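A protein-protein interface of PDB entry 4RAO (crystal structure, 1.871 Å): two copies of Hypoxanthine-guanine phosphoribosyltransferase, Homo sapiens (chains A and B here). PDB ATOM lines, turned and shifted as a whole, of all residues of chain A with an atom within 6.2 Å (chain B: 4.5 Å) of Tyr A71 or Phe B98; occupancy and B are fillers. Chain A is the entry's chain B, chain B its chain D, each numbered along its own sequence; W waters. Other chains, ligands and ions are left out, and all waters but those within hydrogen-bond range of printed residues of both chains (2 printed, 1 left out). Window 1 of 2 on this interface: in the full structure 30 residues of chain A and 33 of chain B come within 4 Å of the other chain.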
ATOM      1  N   CYS A  65      22.558   8.160 -18.242  1.00  0.00           N
ATOM      2  CA  CYS A  65      23.029   7.420 -19.411  1.00  0.00           C
ATOM      3  C   CYS A  65      22.946   8.249 -20.693  1.00  0.00           C
ATOM      4  O   CYS A  65      21.865   8.706 -21.076  1.00  0.00           O
ATOM      5  CB  CYS A  65      22.207   6.148 -19.593  1.00  0.00           C
ATOM      6  SG  CYS A  65      22.739   5.194 -21.035  1.00  0.00           S
ATOM      7  N   VAL A  66      24.081   8.463 -21.357  1.00  0.00           N
ATOM      8  CA  VAL A  66      24.032   9.177 -22.628  1.00  0.00           C
ATOM      9  C   VAL A  66      23.785   8.189 -23.761  1.00  0.00           C
ATOM     10  O   VAL A  66      24.687   7.426 -24.145  1.00  0.00           O
ATOM     11  CB  VAL A  66      25.297  10.003 -22.904  1.00  0.00           C
ATOM     12  CG1 VAL A  66      25.080  10.838 -24.146  1.00  0.00           C
ATOM     13  CG2 VAL A  66      25.616  10.916 -21.718  1.00  0.00           C
ATOM     14  N   LEU A  67      22.554   8.207 -24.278  1.00  0.00           N
ATOM     15  CA  LEU A  67      22.101   7.295 -25.332  1.00  0.00           C
ATOM     16  C   LEU A  67      22.604   7.784 -26.694  1.00  0.00           C
ATOM     17  O   LEU A  67      22.943   8.962 -26.826  1.00  0.00           O
ATOM     18  CB  LEU A  67      20.572   7.212 -25.314  1.00  0.00           C
ATOM     19  CG  LEU A  67      19.930   6.551 -24.091  1.00  0.00           C
ATOM     20  CD1 LEU A  67      18.420   6.685 -24.146  1.00  0.00           C
ATOM     21  CD2 LEU A  67      20.333   5.081 -23.988  1.00  0.00           C
ATOM     22  N   LYS A  68      22.678   6.909 -27.702  1.00  0.00           N
ATOM     23  CA  LYS A  68      22.390   5.478 -27.583  1.00  0.00           C
ATOM     24  C   LYS A  68      23.629   4.711 -27.176  1.00  0.00           C
ATOM     25  O   LYS A  68      23.544   3.680 -26.510  1.00  0.00           O
ATOM     26  CB  LYS A  68      21.933   4.925 -28.934  1.00  0.00           C
ATOM     27  CG  LYS A  68      20.682   5.534 -29.521  1.00  0.00           C
ATOM     28  CD  LYS A  68      20.178   4.615 -30.635  1.00  0.00           C
ATOM     29  CE  LYS A  68      19.410   5.351 -31.685  1.00  0.00           C
ATOM     30  NZ  LYS A  68      19.053   4.424 -32.809  1.00  0.00           N
ATOM     31  N   GLY A  69      24.783   5.209 -27.601  1.00  0.00           N
ATOM     32  CA  GLY A  69      26.038   4.493 -27.443  1.00  0.00           C
ATOM     33  C   GLY A  69      26.472   4.159 -26.025  1.00  0.00           C
ATOM     34  O   GLY A  69      27.231   3.206 -25.803  1.00  0.00           O
ATOM     35  N   GLY A  70      26.014   4.934 -25.052  1.00  0.00           N
ATOM     36  CA  GLY A  70      26.460   4.694 -23.690  1.00  0.00           C
ATOM     37  C   GLY A  70      25.697   3.575 -23.001  1.00  0.00           C
ATOM     38  O   GLY A  70      26.047   3.206 -21.881  1.00  0.00           O
ATOM     39  N   TYR A  71      24.678   3.020 -23.658  1.00  0.00           N
ATOM     40  CA  TYR A  71      23.752   2.119 -22.953  1.00  0.00           C
ATOM     41  C   TYR A  71      24.424   0.857 -22.399  1.00  0.00           C
ATOM     42  O   TYR A  71      24.072   0.383 -21.315  1.00  0.00           O
ATOM     43  CB  TYR A  71      22.505   1.780 -23.812  1.00  0.00           C
ATOM     44  CG  TYR A  71      22.507   0.395 -24.452  1.00  0.00           C
ATOM     45  CD1 TYR A  71      22.102  -0.728 -23.741  1.00  0.00           C
ATOM     46  CD2 TYR A  71      22.888   0.227 -25.780  1.00  0.00           C
ATOM     47  CE1 TYR A  71      22.105  -1.990 -24.333  1.00  0.00           C
ATOM     48  CE2 TYR A  71      22.900  -1.024 -26.375  1.00  0.00           C
ATOM     49  CZ  TYR A  71      22.515  -2.128 -25.639  1.00  0.00           C
ATOM     50  OH  TYR A  71      22.512  -3.376 -26.231  1.00  0.00           O
ATOM     51  N   LYS A  72      25.363   0.281 -23.142  1.00  0.00           N
ATOM     52  CA  LYS A  72      25.991  -0.964 -22.681  1.00  0.00           C
ATOM     53  C   LYS A  72      26.934  -0.700 -21.507  1.00  0.00           C
ATOM     54  O   LYS A  72      26.854  -1.354 -20.461  1.00  0.00           O
ATOM     55  CB  LYS A  72      26.744  -1.653 -23.818  1.00  0.00           C
ATOM     56  CG  LYS A  72      25.884  -2.565 -24.655  1.00  0.00           C
ATOM     57  CD  LYS A  72      25.346  -3.697 -23.814  1.00  0.00           C
ATOM     58  CE  LYS A  72      26.413  -4.729 -23.543  1.00  0.00           C
ATOM     59  NZ  LYS A  72      25.860  -5.838 -22.724  1.00  0.00           N
ATOM     60  N   PHE A  73      27.830   0.261 -21.684  1.00  0.00           N
ATOM     61  CA  PHE A  73      28.749   0.639 -20.621  1.00  0.00           C
ATOM     62  C   PHE A  73      27.965   1.038 -19.362  1.00  0.00           C
ATOM     63  O   PHE A  73      28.319   0.664 -18.239  1.00  0.00           O
ATOM     64  CB  PHE A  73      29.637   1.787 -21.117  1.00  0.00           C
ATOM     65  CG  PHE A  73      30.639   2.263 -20.119  1.00  0.00           C
ATOM     66  CD1 PHE A  73      31.482   1.369 -19.461  1.00  0.00           C
ATOM     67  CD2 PHE A  73      30.767   3.624 -19.856  1.00  0.00           C
ATOM     68  CE1 PHE A  73      32.428   1.830 -18.542  1.00  0.00           C
ATOM     69  CE2 PHE A  73      31.716   4.095 -18.946  1.00  0.00           C
ATOM     70  CZ  PHE A  73      32.549   3.196 -18.294  1.00  0.00           C
ATOM     71  N   PHE A  74      26.879   1.772 -19.554  1.00  0.00           N
ATOM     72  CA  PHE A  74      26.035   2.199 -18.439  1.00  0.00           C
ATOM     73  C   PHE A  74      25.461   0.980 -17.700  1.00  0.00           C
ATOM     74  O   PHE A  74      25.539   0.893 -16.477  1.00  0.00           O
ATOM     75  CB  PHE A  74      24.928   3.111 -18.987  1.00  0.00           C
ATOM     76  CG  PHE A  74      23.916   3.570 -17.953  1.00  0.00           C
ATOM     77  CD1 PHE A  74      24.153   4.702 -17.183  1.00  0.00           C
ATOM     78  CD2 PHE A  74      22.714   2.899 -17.795  1.00  0.00           C
ATOM     79  CE1 PHE A  74      23.212   5.143 -16.248  1.00  0.00           C
ATOM     80  CE2 PHE A  74      21.778   3.330 -16.862  1.00  0.00           C
ATOM     81  CZ  PHE A  74      22.024   4.462 -16.099  1.00  0.00           C
ATOM     82  N   ALA A  75      24.895   0.030 -18.440  1.00  0.00           N
ATOM     83  CA  ALA A  75      24.241  -1.117 -17.799  1.00  0.00           C
ATOM     84  C   ALA A  75      25.262  -1.960 -17.040  1.00  0.00           C
ATOM     85  O   ALA A  75      25.014  -2.402 -15.919  1.00  0.00           O
ATOM     86  CB  ALA A  75      23.495  -1.961 -18.830  1.00  0.00           C
ATOM     87  N   ASP A  76      26.418  -2.165 -17.651  1.00  0.00           N
ATOM     88  CA  ASP A  76      27.464  -2.984 -17.053  1.00  0.00           C
ATOM     89  C   ASP A  76      28.120  -2.266 -15.880  1.00  0.00           C
ATOM     90  O   ASP A  76      28.356  -2.875 -14.840  1.00  0.00           O
ATOM     91  CB  ASP A  76      28.523  -3.354 -18.100  1.00  0.00           C
ATOM     92  CG  ASP A  76      28.008  -4.328 -19.143  1.00  0.00           C
ATOM     93  OD1 ASP A  76      27.013  -5.013 -18.868  1.00  0.00           O
ATOM     94  OD2 ASP A  76      28.619  -4.429 -20.238  1.00  0.00           O
ATOM     95  N   PHE A  98      18.050   8.866 -18.552  1.00  0.00           N
ATOM     96  CA  PHE A  98      18.641   8.594 -19.844  1.00  0.00           C
ATOM     97  C   PHE A  98      18.454   9.851 -20.651  1.00  0.00           C
ATOM     98  O   PHE A  98      17.355  10.400 -20.701  1.00  0.00           O
ATOM     99  CB  PHE A  98      17.898   7.445 -20.530  1.00  0.00           C
ATOM    100  CG  PHE A  98      17.975   6.148 -19.790  1.00  0.00           C
ATOM    101  CD1 PHE A  98      17.072   5.858 -18.767  1.00  0.00           C
ATOM    102  CD2 PHE A  98      18.945   5.212 -20.116  1.00  0.00           C
ATOM    103  CE1 PHE A  98      17.146   4.650 -18.066  1.00  0.00           C
ATOM    104  CE2 PHE A  98      19.030   3.996 -19.430  1.00  0.00           C
ATOM    105  CZ  PHE A  98      18.120   3.716 -18.402  1.00  0.00           C
ATOM    106  N   ARG A 100      19.422  11.838 -24.495  1.00  0.00           N
ATOM    107  CA  ARG A 100      20.024  11.714 -25.807  1.00  0.00           C
ATOM    108  C   ARG A 100      20.173  13.083 -26.424  1.00  0.00           C
ATOM    109  O   ARG A 100      19.350  13.977 -26.203  1.00  0.00           O
ATOM    110  CB  ARG A 100      19.223  10.796 -26.725  1.00  0.00           C
ATOM    111  CG  ARG A 100      20.017  10.351 -27.948  1.00  0.00           C
ATOM    112  CD  ARG A 100      19.117  10.075 -29.134  1.00  0.00           C
ATOM    113  NE  ARG A 100      18.045   9.159 -28.776  1.00  0.00           N
ATOM    114  CZ  ARG A 100      17.332   8.462 -29.653  1.00  0.00           C
ATOM    115  NH1 ARG A 100      17.581   8.570 -30.950  1.00  0.00           N
ATOM    116  NH2 ARG A 100      16.376   7.649 -29.232  1.00  0.00           N
ATOM    117  N   ILE A 116      16.395  14.835 -26.017  1.00  0.00           N
ATOM    118  CA  ILE A 116      15.187  14.060 -25.737  1.00  0.00           C
ATOM    119  C   ILE A 116      15.294  13.345 -24.398  1.00  0.00           C
ATOM    120  O   ILE A 116      16.384  12.930 -23.984  1.00  0.00           O
ATOM    121  CB  ILE A 116      14.806  13.070 -26.877  1.00  0.00           C
ATOM    122  CG1 ILE A 116      14.519  11.668 -26.321  1.00  0.00           C
ATOM    123  CG2 ILE A 116      15.864  13.059 -27.972  1.00  0.00           C
ATOM    124  CD1 ILE A 116      15.697  10.725 -26.266  1.00  0.00           C
ATOM    125  N   ASP A 134      29.909   6.870 -23.795  1.00  0.00           N
ATOM    126  CA  ASP A 134      30.631   5.838 -24.530  1.00  0.00           C
ATOM    127  C   ASP A 134      32.018   6.317 -24.962  1.00  0.00           C
ATOM    128  O   ASP A 134      33.015   5.603 -24.789  1.00  0.00           O
ATOM    129  CB  ASP A 134      29.812   5.319 -25.727  1.00  0.00           C
ATOM    130  CG  ASP A 134      29.378   6.428 -26.688  1.00  0.00           C
ATOM    131  OD1 ASP A 134      29.480   7.622 -26.336  1.00  0.00           O
ATOM    132  OD2 ASP A 134      28.922   6.089 -27.802  1.00  0.00           O
ATOM    133  N   TYR A 190      30.234  -2.803 -28.844  1.00  0.00           N
ATOM    134  CA  TYR A 190      29.826  -2.494 -27.457  1.00  0.00           C
ATOM    135  C   TYR A 190      28.916  -1.255 -27.436  1.00  0.00           C
ATOM    136  O   TYR A 190      29.096  -0.332 -26.627  1.00  0.00           O
ATOM    137  CB  TYR A 190      31.061  -2.327 -26.558  1.00  0.00           C
ATOM    138  CG  TYR A 190      30.793  -2.390 -25.071  1.00  0.00           C
ATOM    139  CD1 TYR A 190      30.407  -3.582 -24.451  1.00  0.00           C
ATOM    140  CD2 TYR A 190      30.944  -1.266 -24.284  1.00  0.00           C
ATOM    141  CE1 TYR A 190      30.170  -3.631 -23.083  1.00  0.00           C
ATOM    142  CE2 TYR A 190      30.715  -1.304 -22.915  1.00  0.00           C
ATOM    143  CZ  TYR A 190      30.330  -2.491 -22.322  1.00  0.00           C
ATOM    144  OH  TYR A 190      30.108  -2.521 -20.961  1.00  0.00           O
ATOM    145  N   ALA A 191      27.944  -1.253 -28.360  1.00  0.00           N
ATOM    146  CA  ALA A 191      26.928  -0.193 -28.523  1.00  0.00           C
ATOM    147  C   ALA A 191      27.351   1.049 -29.324  1.00  0.00           C
ATOM    148  O   ALA A 191      26.498   1.869 -29.665  1.00  0.00           O
ATOM    149  CB  ALA A 191      26.263   0.215 -27.168  1.00  0.00           C
ATOM    150  N   ARG A 199      26.104  -1.891 -33.276  1.00  0.00           N
ATOM    151  CA  ARG A 199      25.787  -1.773 -31.855  1.00  0.00           C
ATOM    152  C   ARG A 199      25.625  -3.159 -31.268  1.00  0.00           C
ATOM    153  O   ARG A 199      25.858  -3.365 -30.071  1.00  0.00           O
ATOM    154  CB  ARG A 199      24.536  -0.935 -31.604  1.00  0.00           C
ATOM    155  CG  ARG A 199      24.660   0.545 -32.048  1.00  0.00           C
ATOM    156  CD  ARG A 199      23.594   1.406 -31.379  1.00  0.00           C
ATOM    157  NE  ARG A 199      23.346   2.697 -32.029  1.00  0.00           N
ATOM    158  CZ  ARG A 199      24.034   3.810 -31.772  1.00  0.00           C
ATOM    159  NH1 ARG A 199      25.019   3.787 -30.889  1.00  0.00           N
ATOM    160  NH2 ARG A 199      23.738   4.943 -32.401  1.00  0.00           N
ATOM    161  N   CYS B  65      13.697  -0.426 -26.941  1.00  0.00           N
ATOM    162  CA  CYS B  65      13.648  -0.473 -25.485  1.00  0.00           C
ATOM    163  C   CYS B  65      12.645   0.548 -24.956  1.00  0.00           C
ATOM    164  O   CYS B  65      12.749   1.748 -25.252  1.00  0.00           O
ATOM    165  CB  CYS B  65      15.030  -0.172 -24.920  1.00  0.00           C
ATOM    166  SG  CYS B  65      15.115  -0.129 -23.124  1.00  0.00           S
ATOM    167  N   LEU B  67      11.914   2.626 -22.159  1.00  0.00           N
ATOM    168  CA  LEU B  67      12.533   3.210 -20.958  1.00  0.00           C
ATOM    169  C   LEU B  67      11.463   3.619 -19.956  1.00  0.00           C
ATOM    170  O   LEU B  67      10.309   3.772 -20.351  1.00  0.00           O
ATOM    171  CB  LEU B  67      13.340   4.446 -21.371  1.00  0.00           C
ATOM    172  CG  LEU B  67      14.606   4.201 -22.179  1.00  0.00           C
ATOM    173  CD1 LEU B  67      15.178   5.538 -22.633  1.00  0.00           C
ATOM    174  CD2 LEU B  67      15.611   3.424 -21.344  1.00  0.00           C
ATOM    175  N   PHE B  74      15.980  -5.351 -21.414  1.00  0.00           N
ATOM    176  CA  PHE B  74      16.452  -5.066 -22.766  1.00  0.00           C
ATOM    177  C   PHE B  74      17.934  -5.411 -22.919  1.00  0.00           C
ATOM    178  O   PHE B  74      18.313  -6.108 -23.865  1.00  0.00           O
ATOM    179  CB  PHE B  74      16.170  -3.584 -23.121  1.00  0.00           C
ATOM    180  CG  PHE B  74      16.690  -3.142 -24.486  1.00  0.00           C
ATOM    181  CD1 PHE B  74      15.939  -3.345 -25.645  1.00  0.00           C
ATOM    182  CD2 PHE B  74      17.903  -2.463 -24.590  1.00  0.00           C
ATOM    183  CE1 PHE B  74      16.401  -2.899 -26.894  1.00  0.00           C
ATOM    184  CE2 PHE B  74      18.380  -2.022 -25.829  1.00  0.00           C
ATOM    185  CZ  PHE B  74      17.625  -2.232 -26.983  1.00  0.00           C
ATOM    186  N   ALA B  75      18.776  -4.931 -22.005  1.00  0.00           N
ATOM    187  CA  ALA B  75      20.220  -5.146 -22.151  1.00  0.00           C
ATOM    188  C   ALA B  75      20.516  -6.634 -22.112  1.00  0.00           C
ATOM    189  O   ALA B  75      21.333  -7.140 -22.884  1.00  0.00           O
ATOM    190  CB  ALA B  75      20.996  -4.441 -21.058  1.00  0.00           C
ATOM    191  N   LEU B  78      19.014  -8.695 -25.141  1.00  0.00           N
ATOM    192  CA  LEU B  78      19.870  -8.479 -26.307  1.00  0.00           C
ATOM    193  C   LEU B  78      21.223  -9.182 -26.193  1.00  0.00           C
ATOM    194  O   LEU B  78      21.754  -9.685 -27.198  1.00  0.00           O
ATOM    195  CB  LEU B  78      20.059  -6.985 -26.628  1.00  0.00           C
ATOM    196  CG  LEU B  78      19.154  -6.453 -27.726  1.00  0.00           C
ATOM    197  CD1 LEU B  78      17.701  -6.659 -27.323  1.00  0.00           C
ATOM    198  CD2 LEU B  78      19.447  -4.976 -27.998  1.00  0.00           C
ATOM    199  N   LYS B  82      22.665 -11.665 -28.885  1.00  0.00           N
ATOM    200  CA  LYS B  82      24.012 -11.526 -29.472  1.00  0.00           C
ATOM    201  C   LYS B  82      24.853 -12.793 -29.315  1.00  0.00           C
ATOM    202  O   LYS B  82      25.588 -13.197 -30.227  1.00  0.00           O
ATOM    203  CB  LYS B  82      24.750 -10.332 -28.864  1.00  0.00           C
ATOM    204  CG  LYS B  82      24.302  -8.994 -29.469  1.00  0.00           C
ATOM    205  CD  LYS B  82      24.234  -7.894 -28.419  1.00  0.00           C
ATOM    206  CE  LYS B  82      25.580  -7.672 -27.773  1.00  0.00           C
ATOM    207  NZ  LYS B  82      25.491  -6.616 -26.720  1.00  0.00           N
ATOM    208  N   VAL B  96      19.240  -0.819 -32.670  1.00  0.00           N
ATOM    209  CA  VAL B  96      18.500  -0.538 -31.438  1.00  0.00           C
ATOM    210  C   VAL B  96      17.962   0.889 -31.398  1.00  0.00           C
ATOM    211  O   VAL B  96      18.513   1.792 -32.025  1.00  0.00           O
ATOM    212  CB  VAL B  96      19.347  -0.810 -30.169  1.00  0.00           C
ATOM    213  CG1 VAL B  96      19.911  -2.206 -30.188  1.00  0.00           C
ATOM    214  CG2 VAL B  96      20.470   0.197 -30.044  1.00  0.00           C
ATOM    215  N   ASP B  97      16.863   1.076 -30.669  1.00  0.00           N
ATOM    216  CA  ASP B  97      16.365   2.410 -30.381  1.00  0.00           C
ATOM    217  C   ASP B  97      15.724   2.394 -28.995  1.00  0.00           C
ATOM    218  O   ASP B  97      15.487   1.324 -28.408  1.00  0.00           O
ATOM    219  CB  ASP B  97      15.377   2.888 -31.447  1.00  0.00           C
ATOM    220  CG  ASP B  97      15.290   4.417 -31.526  1.00  0.00           C
ATOM    221  OD1 ASP B  97      16.065   5.116 -30.814  1.00  0.00           O
ATOM    222  OD2 ASP B  97      14.447   4.916 -32.303  1.00  0.00           O
ATOM    223  N   PHE B  98      15.476   3.586 -28.477  1.00  0.00           N
ATOM    224  CA  PHE B  98      14.932   3.765 -27.140  1.00  0.00           C
ATOM    225  C   PHE B  98      13.801   4.764 -27.194  1.00  0.00           C
ATOM    226  O   PHE B  98      13.946   5.859 -27.745  1.00  0.00           O
ATOM    227  CB  PHE B  98      16.018   4.289 -26.203  1.00  0.00           C
ATOM    228  CG  PHE B  98      17.215   3.410 -26.133  1.00  0.00           C
ATOM    229  CD1 PHE B  98      18.221   3.502 -27.094  1.00  0.00           C
ATOM    230  CD2 PHE B  98      17.347   2.477 -25.105  1.00  0.00           C
ATOM    231  CE1 PHE B  98      19.322   2.681 -27.042  1.00  0.00           C
ATOM    232  CE2 PHE B  98      18.441   1.650 -25.050  1.00  0.00           C
ATOM    233  CZ  PHE B  98      19.436   1.746 -26.017  1.00  0.00           C
ATOM    234  N   ILE B  99      12.667   4.394 -26.622  1.00  0.00           N
ATOM    235  CA  ILE B  99      11.556   5.320 -26.531  1.00  0.00           C
ATOM    236  C   ILE B  99      11.025   5.371 -25.110  1.00  0.00           C
ATOM    237  O   ILE B  99      11.284   4.484 -24.298  1.00  0.00           O
ATOM    238  CB  ILE B  99      10.429   4.933 -27.488  1.00  0.00           C
ATOM    239  CG1 ILE B  99       9.885   3.554 -27.125  1.00  0.00           C
ATOM    240  CG2 ILE B  99      10.922   4.972 -28.940  1.00  0.00           C
ATOM    241  CD1 ILE B  99       8.781   3.092 -28.030  1.00  0.00           C
ATOM    242  N   GLY B 117      10.924  10.774 -27.781  1.00  0.00           N
ATOM    243  CA  GLY B 117      12.225  10.369 -28.268  1.00  0.00           C
ATOM    244  C   GLY B 117      12.183   9.266 -29.298  1.00  0.00           C
ATOM    245  O   GLY B 117      11.173   9.069 -29.981  1.00  0.00           O
ATOM    246  N   GLY B 118      13.288   8.535 -29.400  1.00  0.00           N
ATOM    247  CA  GLY B 118      13.424   7.520 -30.422  1.00  0.00           C
ATOM    248  C   GLY B 118      13.929   8.142 -31.708  1.00  0.00           C
ATOM    249  O   GLY B 118      13.999   9.373 -31.838  1.00  0.00           O
HETATM  250  O   HOH W   1      22.762  -5.629 -24.509  1.00  0.00           O
HETATM  251  O   HOH W   2      21.173   0.870 -33.746  1.00  0.00           O
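Among the printed residues, pairs that only touch across the chains: Leu A67 with Leu B67 (3.8 Å), Leu A67 with Phe B98 (3.97 Å), Lys A68 with Phe B98 (3.9 Å), Tyr A71 with Leu B78 (3.9 Å), Tyr A71 with Phe B98 (3.7 Å), Lys A72 with Lys B82 (3.8 Å), Phe A98 with Leu B67 (3.8 Å), Ile A116 with Gly B117 (3.3 Å) and Arg A199 with Val B96 (3.6 Å).
Printed residues of chain B within 4 Å of Leu A67: Leu B67 (3.8 Å) and Phe B98 (3.97 Å).
Printed residues of chain B within 4 Å of Tyr A71: Leu B78 (3.9 Å) and Phe B98 (3.7 Å).
Phe A73 touches none of the printed residues of chain B.
Phe A74 touches none of the printed residues of chain B.
Printed residues of chain A within 4 Å of Val B96: Lys A68 and Arg A199.
Of the printed residues of chain A, Asp B97 touches Lys A68 and Arg A100.
Of the printed residues of chain A, Phe B98 touches Leu A67 (3.97 Å), Lys A68 (3.9 Å), Tyr A71 (3.7 Å) and Arg A100 (3.4 Å).
Printed residues of chain A within 4 Å of Gly B118: Arg A100.
The side-chain amino group of Lys A68 is in hydrogen-bond range of the backbone carbonyl oxygen of Val B96 (2.8 Å).
O of Phe B98 sits at hydrogen-bond distance from NH2 of Arg A100 (3.4 Å).
The guanidinium group (NH2) of Arg A100 lies within salt-bridge range of the side-chain carboxylate (OD1) of Asp B97 (3.0 Å).
The guanidinium group (NH2) of Arg A100 sits close to the backbone NH (N) of Gly B118 (3.2 Å).
The side-chain carboxylate (OD1) of Asp B97 is in salt-bridge range of the side-chain amino group (NZ) of Lys A68.
Leu A67 touches its own counterpart, Leu B67.
Leu A67 touches Phe B98, and with the chains exchanged Phe A98 touches Leu B67.
Positions printed for both chains: 65, 67, 74, 75 and 98.
Water W1 bridges O of Ala B75 (2.6 Å) and OH of Tyr A71 (2.8 Å).
Water W2 lies within hydrogen-bond range of the backbone NH of Val B96 (2.8 Å) and the guanidinium group of Arg A199 (3.3 Å).
The backbone carbonyl oxygen of Phe B98 sits close to the backbone NH of Gly B118, at 3.2 Å.
The guanidinium group of Arg A199 lies within hydrogen-bond range of the backbone carbonyl oxygen of Ala A191 (2.7 Å).
The side-chain amino group (NZ) of Lys A72 is in salt-bridge range of the side-chain carboxylate (OD2) of Asp A76.
OH of Tyr A190 is in hydrogen-bond range of O of Lys A72, at 3.5 Å.
The backbone carbonyl oxygen (O) of Asp B97 is in hydrogen-bond range of the backbone NH (N) of Cys B65, 2.9 Å away.
N of Leu B67 sits at hydrogen-bond distance from O of Ile B99.
Of the 12 printed residues of chain B, 8 touch a printed residue of chain A.
Printed residues of chain B that touch a printed residue of chain A: Leu B67, Leu B78, Lys B82, Val B96, Asp B97, Phe B98, Gly B117 and Gly B118.
Hydrophobic or aromatic side chains of chain B within 4 Å of the printed part of chain A: Leu B67, Leu B78, Val B96 and Phe B98.
Along chain B the printed residues that touch a printed residue of chain A span positions 67 to 118.
Hydrophobic or aromatic side chains of chain A that line the printed part of chain B: Leu A67, Tyr A71, Phe A98 and Ile A116.
Among the printed residues, Asp or Glu carboxylates within 4 Å of a Lys or Arg side-chain nitrogen of the other chain: Lys A68 with Asp B97 (3.7 Å) and Arg A100 with Asp B97 (3.0 Å).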
